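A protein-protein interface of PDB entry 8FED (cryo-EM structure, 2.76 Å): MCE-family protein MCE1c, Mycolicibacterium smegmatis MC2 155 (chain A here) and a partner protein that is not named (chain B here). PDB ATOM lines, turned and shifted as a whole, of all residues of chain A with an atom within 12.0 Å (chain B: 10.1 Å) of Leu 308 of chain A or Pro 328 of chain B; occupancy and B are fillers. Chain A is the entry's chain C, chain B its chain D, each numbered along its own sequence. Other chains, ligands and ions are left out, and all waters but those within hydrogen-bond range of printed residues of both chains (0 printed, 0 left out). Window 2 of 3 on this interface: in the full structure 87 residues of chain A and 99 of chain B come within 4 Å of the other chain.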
ATOM      1  N   ALA A 297      21.284  -1.549 -25.596  1.00  0.00           N
ATOM      2  CA  ALA A 297      20.683  -2.867 -25.797  1.00  0.00           C
ATOM      3  C   ALA A 297      19.181  -2.839 -25.562  1.00  0.00           C
ATOM      4  O   ALA A 297      18.406  -3.411 -26.335  1.00  0.00           O
ATOM      5  CB  ALA A 297      21.347  -3.894 -24.882  1.00  0.00           C
ATOM      6  N   LEU A 298      18.757  -2.170 -24.498  1.00  0.00           N
ATOM      7  CA  LEU A 298      17.348  -2.036 -24.136  1.00  0.00           C
ATOM      8  C   LEU A 298      16.717  -0.772 -24.735  1.00  0.00           C
ATOM      9  O   LEU A 298      16.153   0.084 -24.061  1.00  0.00           O
ATOM     10  CB  LEU A 298      17.238  -2.149 -22.617  1.00  0.00           C
ATOM     11  CG  LEU A 298      17.902  -1.221 -21.582  1.00  0.00           C
ATOM     12  CD1 LEU A 298      17.262   0.108 -21.270  1.00  0.00           C
ATOM     13  CD2 LEU A 298      18.135  -2.020 -20.311  1.00  0.00           C
ATOM     14  N   SER A 300      15.485  -1.162 -28.470  1.00  0.00           N
ATOM     15  CA  SER A 300      14.697  -1.599 -29.620  1.00  0.00           C
ATOM     16  C   SER A 300      13.217  -1.721 -29.280  1.00  0.00           C
ATOM     17  O   SER A 300      12.357  -1.274 -30.047  1.00  0.00           O
ATOM     18  CB  SER A 300      15.237  -2.927 -30.150  1.00  0.00           C
ATOM     19  OG  SER A 300      16.580  -2.800 -30.579  1.00  0.00           O
ATOM     20  N   GLY A 301      12.898  -2.323 -28.137  1.00  0.00           N
ATOM     21  CA  GLY A 301      11.520  -2.529 -27.758  1.00  0.00           C
ATOM     22  C   GLY A 301      11.325  -2.542 -26.256  1.00  0.00           C
ATOM     23  O   GLY A 301      12.234  -2.210 -25.488  1.00  0.00           O
ATOM     24  N   PRO A 302      10.124  -2.919 -25.801  1.00  0.00           N
ATOM     25  CA  PRO A 302       9.875  -3.085 -24.356  1.00  0.00           C
ATOM     26  C   PRO A 302      10.470  -4.380 -23.809  1.00  0.00           C
ATOM     27  O   PRO A 302       9.771  -5.241 -23.270  1.00  0.00           O
ATOM     28  CB  PRO A 302       8.344  -3.059 -24.283  1.00  0.00           C
ATOM     29  CG  PRO A 302       7.901  -3.576 -25.592  1.00  0.00           C
ATOM     30  CD  PRO A 302       8.893  -3.067 -26.594  1.00  0.00           C
ATOM     31  N   TYR A 303      11.780  -4.515 -23.952  1.00  0.00           N
ATOM     32  CA  TYR A 303      12.541  -5.691 -23.539  1.00  0.00           C
ATOM     33  C   TYR A 303      14.018  -5.317 -23.605  1.00  0.00           C
ATOM     34  O   TYR A 303      14.367  -4.156 -23.847  1.00  0.00           O
ATOM     35  CB  TYR A 303      12.213  -6.905 -24.411  1.00  0.00           C
ATOM     36  CG  TYR A 303      11.843  -6.561 -25.838  1.00  0.00           C
ATOM     37  CD1 TYR A 303      12.811  -6.195 -26.763  1.00  0.00           C
ATOM     38  CD2 TYR A 303      10.522  -6.606 -26.259  1.00  0.00           C
ATOM     39  CE1 TYR A 303      12.471  -5.884 -28.065  1.00  0.00           C
ATOM     40  CE2 TYR A 303      10.174  -6.293 -27.556  1.00  0.00           C
ATOM     41  CZ  TYR A 303      11.150  -5.934 -28.453  1.00  0.00           C
ATOM     42  OH  TYR A 303      10.798  -5.625 -29.744  1.00  0.00           O
ATOM     43  N   PHE A 304      14.890  -6.296 -23.386  1.00  0.00           N
ATOM     44  CA  PHE A 304      16.323  -6.100 -23.560  1.00  0.00           C
ATOM     45  C   PHE A 304      16.928  -7.359 -24.156  1.00  0.00           C
ATOM     46  O   PHE A 304      16.618  -8.469 -23.716  1.00  0.00           O
ATOM     47  CB  PHE A 304      17.005  -5.740 -22.231  1.00  0.00           C
ATOM     48  CG  PHE A 304      16.949  -6.826 -21.194  1.00  0.00           C
ATOM     49  CD1 PHE A 304      15.823  -6.994 -20.410  1.00  0.00           C
ATOM     50  CD2 PHE A 304      18.033  -7.662 -20.985  1.00  0.00           C
ATOM     51  CE1 PHE A 304      15.772  -7.987 -19.456  1.00  0.00           C
ATOM     52  CE2 PHE A 304      17.985  -8.652 -20.029  1.00  0.00           C
ATOM     53  CZ  PHE A 304      16.855  -8.816 -19.267  1.00  0.00           C
ATOM     54  N   LYS A 305      17.782  -7.191 -25.157  1.00  0.00           N
ATOM     55  CA  LYS A 305      18.369  -8.339 -25.826  1.00  0.00           C
ATOM     56  C   LYS A 305      19.422  -9.000 -24.947  1.00  0.00           C
ATOM     57  O   LYS A 305      20.073  -8.353 -24.125  1.00  0.00           O
ATOM     58  CB  LYS A 305      18.978  -7.921 -27.159  1.00  0.00           C
ATOM     59  CG  LYS A 305      18.016  -7.161 -28.050  1.00  0.00           C
ATOM     60  CD  LYS A 305      18.641  -6.835 -29.388  1.00  0.00           C
ATOM     61  CE  LYS A 305      17.851  -5.756 -30.092  1.00  0.00           C
ATOM     62  NZ  LYS A 305      16.401  -6.062 -30.050  1.00  0.00           N
ATOM     63  N   VAL A 306      19.580 -10.310 -25.127  1.00  0.00           N
ATOM     64  CA  VAL A 306      20.565 -11.101 -24.396  1.00  0.00           C
ATOM     65  C   VAL A 306      21.186 -12.110 -25.350  1.00  0.00           C
ATOM     66  O   VAL A 306      20.509 -12.640 -26.237  1.00  0.00           O
ATOM     67  CB  VAL A 306      19.946 -11.821 -23.181  1.00  0.00           C
ATOM     68  CG1 VAL A 306      19.701 -10.849 -22.053  1.00  0.00           C
ATOM     69  CG2 VAL A 306      18.653 -12.508 -23.573  1.00  0.00           C
ATOM     70  N   MET A 307      22.475 -12.370 -25.175  1.00  0.00           N
ATOM     71  CA  MET A 307      23.195 -13.356 -25.976  1.00  0.00           C
ATOM     72  C   MET A 307      23.451 -14.575 -25.092  1.00  0.00           C
ATOM     73  O   MET A 307      24.480 -14.673 -24.423  1.00  0.00           O
ATOM     74  CB  MET A 307      24.498 -12.782 -26.522  1.00  0.00           C
ATOM     75  CG  MET A 307      25.303 -13.765 -27.359  1.00  0.00           C
ATOM     76  SD  MET A 307      26.946 -13.160 -27.783  1.00  0.00           S
ATOM     77  CE  MET A 307      27.597 -14.560 -28.688  1.00  0.00           C
ATOM     78  N   LEU A 308      22.503 -15.505 -25.091  1.00  0.00           N
ATOM     79  CA  LEU A 308      22.642 -16.741 -24.326  1.00  0.00           C
ATOM     80  C   LEU A 308      23.647 -17.631 -25.043  1.00  0.00           C
ATOM     81  O   LEU A 308      23.309 -18.311 -26.013  1.00  0.00           O
ATOM     82  CB  LEU A 308      21.293 -17.436 -24.185  1.00  0.00           C
ATOM     83  CG  LEU A 308      20.070 -16.546 -23.948  1.00  0.00           C
ATOM     84  CD1 LEU A 308      18.799 -17.374 -23.982  1.00  0.00           C
ATOM     85  CD2 LEU A 308      20.183 -15.805 -22.631  1.00  0.00           C
ATOM     86  N   VAL A 309      24.899 -17.612 -24.579  1.00  0.00           N
ATOM     87  CA  VAL A 309      25.945 -18.402 -25.224  1.00  0.00           C
ATOM     88  C   VAL A 309      25.637 -19.890 -25.119  1.00  0.00           C
ATOM     89  O   VAL A 309      25.758 -20.636 -26.100  1.00  0.00           O
ATOM     90  CB  VAL A 309      27.321 -18.061 -24.621  1.00  0.00           C
ATOM     91  CG1 VAL A 309      28.392 -18.990 -25.169  1.00  0.00           C
ATOM     92  CG2 VAL A 309      27.677 -16.611 -24.907  1.00  0.00           C
ATOM     93  N   ASN A 310      25.222 -20.344 -23.942  1.00  0.00           N
ATOM     94  CA  ASN A 310      24.890 -21.749 -23.746  1.00  0.00           C
ATOM     95  C   ASN A 310      23.428 -22.028 -24.083  1.00  0.00           C
ATOM     96  O   ASN A 310      22.941 -23.144 -23.901  1.00  0.00           O
ATOM     97  CB  ASN A 310      25.189 -22.172 -22.308  1.00  0.00           C
ATOM     98  CG  ASN A 310      26.652 -22.027 -21.955  1.00  0.00           C
ATOM     99  OD1 ASN A 310      27.522 -22.096 -22.823  1.00  0.00           O
ATOM    100  ND2 ASN A 310      26.934 -21.825 -20.676  1.00  0.00           N
ATOM    101  N   ILE B 324      11.690  -8.754 -15.500  1.00  0.00           N
ATOM    102  CA  ILE B 324      12.107  -8.082 -16.724  1.00  0.00           C
ATOM    103  C   ILE B 324      12.121  -9.093 -17.861  1.00  0.00           C
ATOM    104  O   ILE B 324      12.510 -10.252 -17.675  1.00  0.00           O
ATOM    105  CB  ILE B 324      13.489  -7.414 -16.566  1.00  0.00           C
ATOM    106  CG1 ILE B 324      14.510  -8.409 -16.017  1.00  0.00           C
ATOM    107  CG2 ILE B 324      13.387  -6.200 -15.664  1.00  0.00           C
ATOM    108  CD1 ILE B 324      15.874  -7.809 -15.780  1.00  0.00           C
ATOM    109  N   ILE B 325      11.682  -8.653 -19.037  1.00  0.00           N
ATOM    110  CA  ILE B 325      11.542  -9.507 -20.210  1.00  0.00           C
ATOM    111  C   ILE B 325      12.778  -9.347 -21.082  1.00  0.00           C
ATOM    112  O   ILE B 325      13.099  -8.236 -21.516  1.00  0.00           O
ATOM    113  CB  ILE B 325      10.273  -9.162 -21.003  1.00  0.00           C
ATOM    114  CG1 ILE B 325       9.043  -9.243 -20.103  1.00  0.00           C
ATOM    115  CG2 ILE B 325      10.130 -10.089 -22.194  1.00  0.00           C
ATOM    116  CD1 ILE B 325       7.759  -8.902 -20.813  1.00  0.00           C
ATOM    117  N   GLY B 326      13.469 -10.449 -21.349  1.00  0.00           N
ATOM    118  CA  GLY B 326      14.636 -10.388 -22.203  1.00  0.00           C
ATOM    119  C   GLY B 326      14.576 -11.354 -23.366  1.00  0.00           C
ATOM    120  O   GLY B 326      14.640 -12.568 -23.169  1.00  0.00           O
ATOM    121  N   LEU B 327      14.471 -10.829 -24.586  1.00  0.00           N
ATOM    122  CA  LEU B 327      14.408 -11.804 -25.670  1.00  0.00           C
ATOM    123  C   LEU B 327      15.810 -12.197 -26.127  1.00  0.00           C
ATOM    124  O   LEU B 327      16.711 -11.356 -26.162  1.00  0.00           O
ATOM    125  CB  LEU B 327      13.618 -11.252 -26.855  1.00  0.00           C
ATOM    126  CG  LEU B 327      13.467  -9.742 -27.058  1.00  0.00           C
ATOM    127  CD1 LEU B 327      14.781  -9.088 -27.428  1.00  0.00           C
ATOM    128  CD2 LEU B 327      12.427  -9.476 -28.129  1.00  0.00           C
ATOM    129  N   PRO B 328      16.019 -13.465 -26.470  1.00  0.00           N
ATOM    130  CA  PRO B 328      17.330 -13.887 -26.967  1.00  0.00           C
ATOM    131  C   PRO B 328      17.568 -13.395 -28.386  1.00  0.00           C
ATOM    132  O   PRO B 328      16.651 -12.986 -29.098  1.00  0.00           O
ATOM    133  CB  PRO B 328      17.252 -15.414 -26.915  1.00  0.00           C
ATOM    134  CG  PRO B 328      15.807 -15.704 -27.098  1.00  0.00           C
ATOM    135  CD  PRO B 328      15.066 -14.586 -26.412  1.00  0.00           C
ATOM    136  N   VAL B 329      18.835 -13.429 -28.787  1.00  0.00           N
ATOM    137  CA  VAL B 329      19.213 -13.049 -30.143  1.00  0.00           C
ATOM    138  C   VAL B 329      20.102 -14.123 -30.753  1.00  0.00           C
ATOM    139  O   VAL B 329      19.903 -14.529 -31.899  1.00  0.00           O
ATOM    140  CB  VAL B 329      19.918 -11.681 -30.180  1.00  0.00           C
ATOM    141  CG1 VAL B 329      18.996 -10.584 -29.670  1.00  0.00           C
ATOM    142  CG2 VAL B 329      21.205 -11.727 -29.376  1.00  0.00           C
ATOM    143  N   TYR B 377      23.191 -12.699 -39.001  1.00  0.00           N
ATOM    144  CA  TYR B 377      22.007 -13.327 -38.417  1.00  0.00           C
ATOM    145  C   TYR B 377      21.091 -13.787 -39.547  1.00  0.00           C
ATOM    146  O   TYR B 377      21.374 -13.576 -40.730  1.00  0.00           O
ATOM    147  CB  TYR B 377      21.285 -12.381 -37.453  1.00  0.00           C
ATOM    148  CG  TYR B 377      20.931 -11.032 -38.032  1.00  0.00           C
ATOM    149  CD1 TYR B 377      21.808  -9.961 -37.933  1.00  0.00           C
ATOM    150  CD2 TYR B 377      19.712 -10.822 -38.658  1.00  0.00           C
ATOM    151  CE1 TYR B 377      21.485  -8.727 -38.452  1.00  0.00           C
ATOM    152  CE2 TYR B 377      19.382  -9.593 -39.180  1.00  0.00           C
ATOM    153  CZ  TYR B 377      20.269  -8.548 -39.074  1.00  0.00           C
ATOM    154  OH  TYR B 377      19.938  -7.319 -39.596  1.00  0.00           O
ATOM    155  N   GLY B 381      12.694 -13.110 -39.597  1.00  0.00           N
ATOM    156  CA  GLY B 381      12.364 -13.053 -38.186  1.00  0.00           C
ATOM    157  C   GLY B 381      10.865 -13.016 -37.991  1.00  0.00           C
ATOM    158  O   GLY B 381      10.120 -12.521 -38.839  1.00  0.00           O
ATOM    159  N   MET B 382      10.426 -13.544 -36.851  1.00  0.00           N
ATOM    160  CA  MET B 382       9.009 -13.702 -36.570  1.00  0.00           C
ATOM    161  C   MET B 382       8.680 -13.157 -35.188  1.00  0.00           C
ATOM    162  O   MET B 382       9.514 -13.166 -34.279  1.00  0.00           O
ATOM    163  CB  MET B 382       8.584 -15.175 -36.664  1.00  0.00           C
ATOM    164  CG  MET B 382       7.112 -15.381 -36.976  1.00  0.00           C
ATOM    165  SD  MET B 382       6.708 -17.100 -37.330  1.00  0.00           S
ATOM    166  CE  MET B 382       5.192 -16.900 -38.264  1.00  0.00           C
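N of Phe 304 of chain A sits close to O of Ile 325 of chain B. The backbone carbonyl oxygen (O) of Phe 304 of chain A sits at hydrogen-bond distance from the backbone NH (N) of Leu 327 of chain B, 3.3 Å away. N of Val 306 of chain A is in hydrogen-bond range of O of Leu 327 of chain B, at 3.2 Å. N of Val 329 of chain B lies within hydrogen-bond range of O of Val 306 of chain A (3.2 Å).
The side-chain amino group of Lys 305 of chain A sits close to the side-chain hydroxyl of Ser 300 of chain A (3.3 Å).
Among the printed residues, pairs that only touch across the chains: Tyr 303 of chain A with Ile 325 of chain B (3.3 Å), Tyr 303 of chain A with Leu 327 of chain B (3.6 Å), Phe 304 of chain A with Ile 324 of chain B (3.7 Å), Phe 304 of chain A with Gly 326 of chain B (3.1 Å), Lys 305 of chain A with Leu 327 of chain B (3.5 Å), Lys 305 of chain A with Val 329 of chain B (3.7 Å), Val 306 of chain A with Pro 328 of chain B (3.5 Å) and Leu 308 of chain A with Pro 328 of chain B (3.9 Å).
Gly 301 of chain A touches none of the printed residues of chain B. Val 306 of chain A touches just these residues of chain B: Leu 327 (3.2 Å), Pro 328 (3.5 Å) and Val 329 (3.2 Å). No residue of chain B comes within 4 Å of Val 309 of chain A. Of the printed residues of chain A, Ile 324 of chain B touches Phe 304 (3.7 Å). Of the printed residues of chain A, Ile 325 of chain B touches Tyr 303 and Phe 304. Leu 327 of chain B touches four residues of chain A. Pro 328 of chain B touches just these residues of chain A: Val 306 (3.5 Å) and Leu 308 (3.9 Å). Val 329 of chain B touches two residues of chain A. Met 382 of chain B touches none of the printed residues of chain A. The nearest printed residue of chain A that does not touch Pro 328 of chain B is Met 307 of chain A (5.7 Å).
Hydrophobic or aromatic side chains of chain A that line the printed part of chain B: Tyr 303, Phe 304, Val 306 and Leu 308. Along chain A the printed residues that touch a printed residue of chain B span positions 303 to 308. Printed residues of chain B that touch a printed residue of chain A: Ile 324, Ile 325, Gly 326, Leu 327, Pro 328 and Val 329. Hydrophobic or aromatic side chains of chain B within 4 Å of the printed part of chain A: Ile 324, Leu 327, Pro 328 and Val 329. Among the printed residues, 12 pairs touch across the chains.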
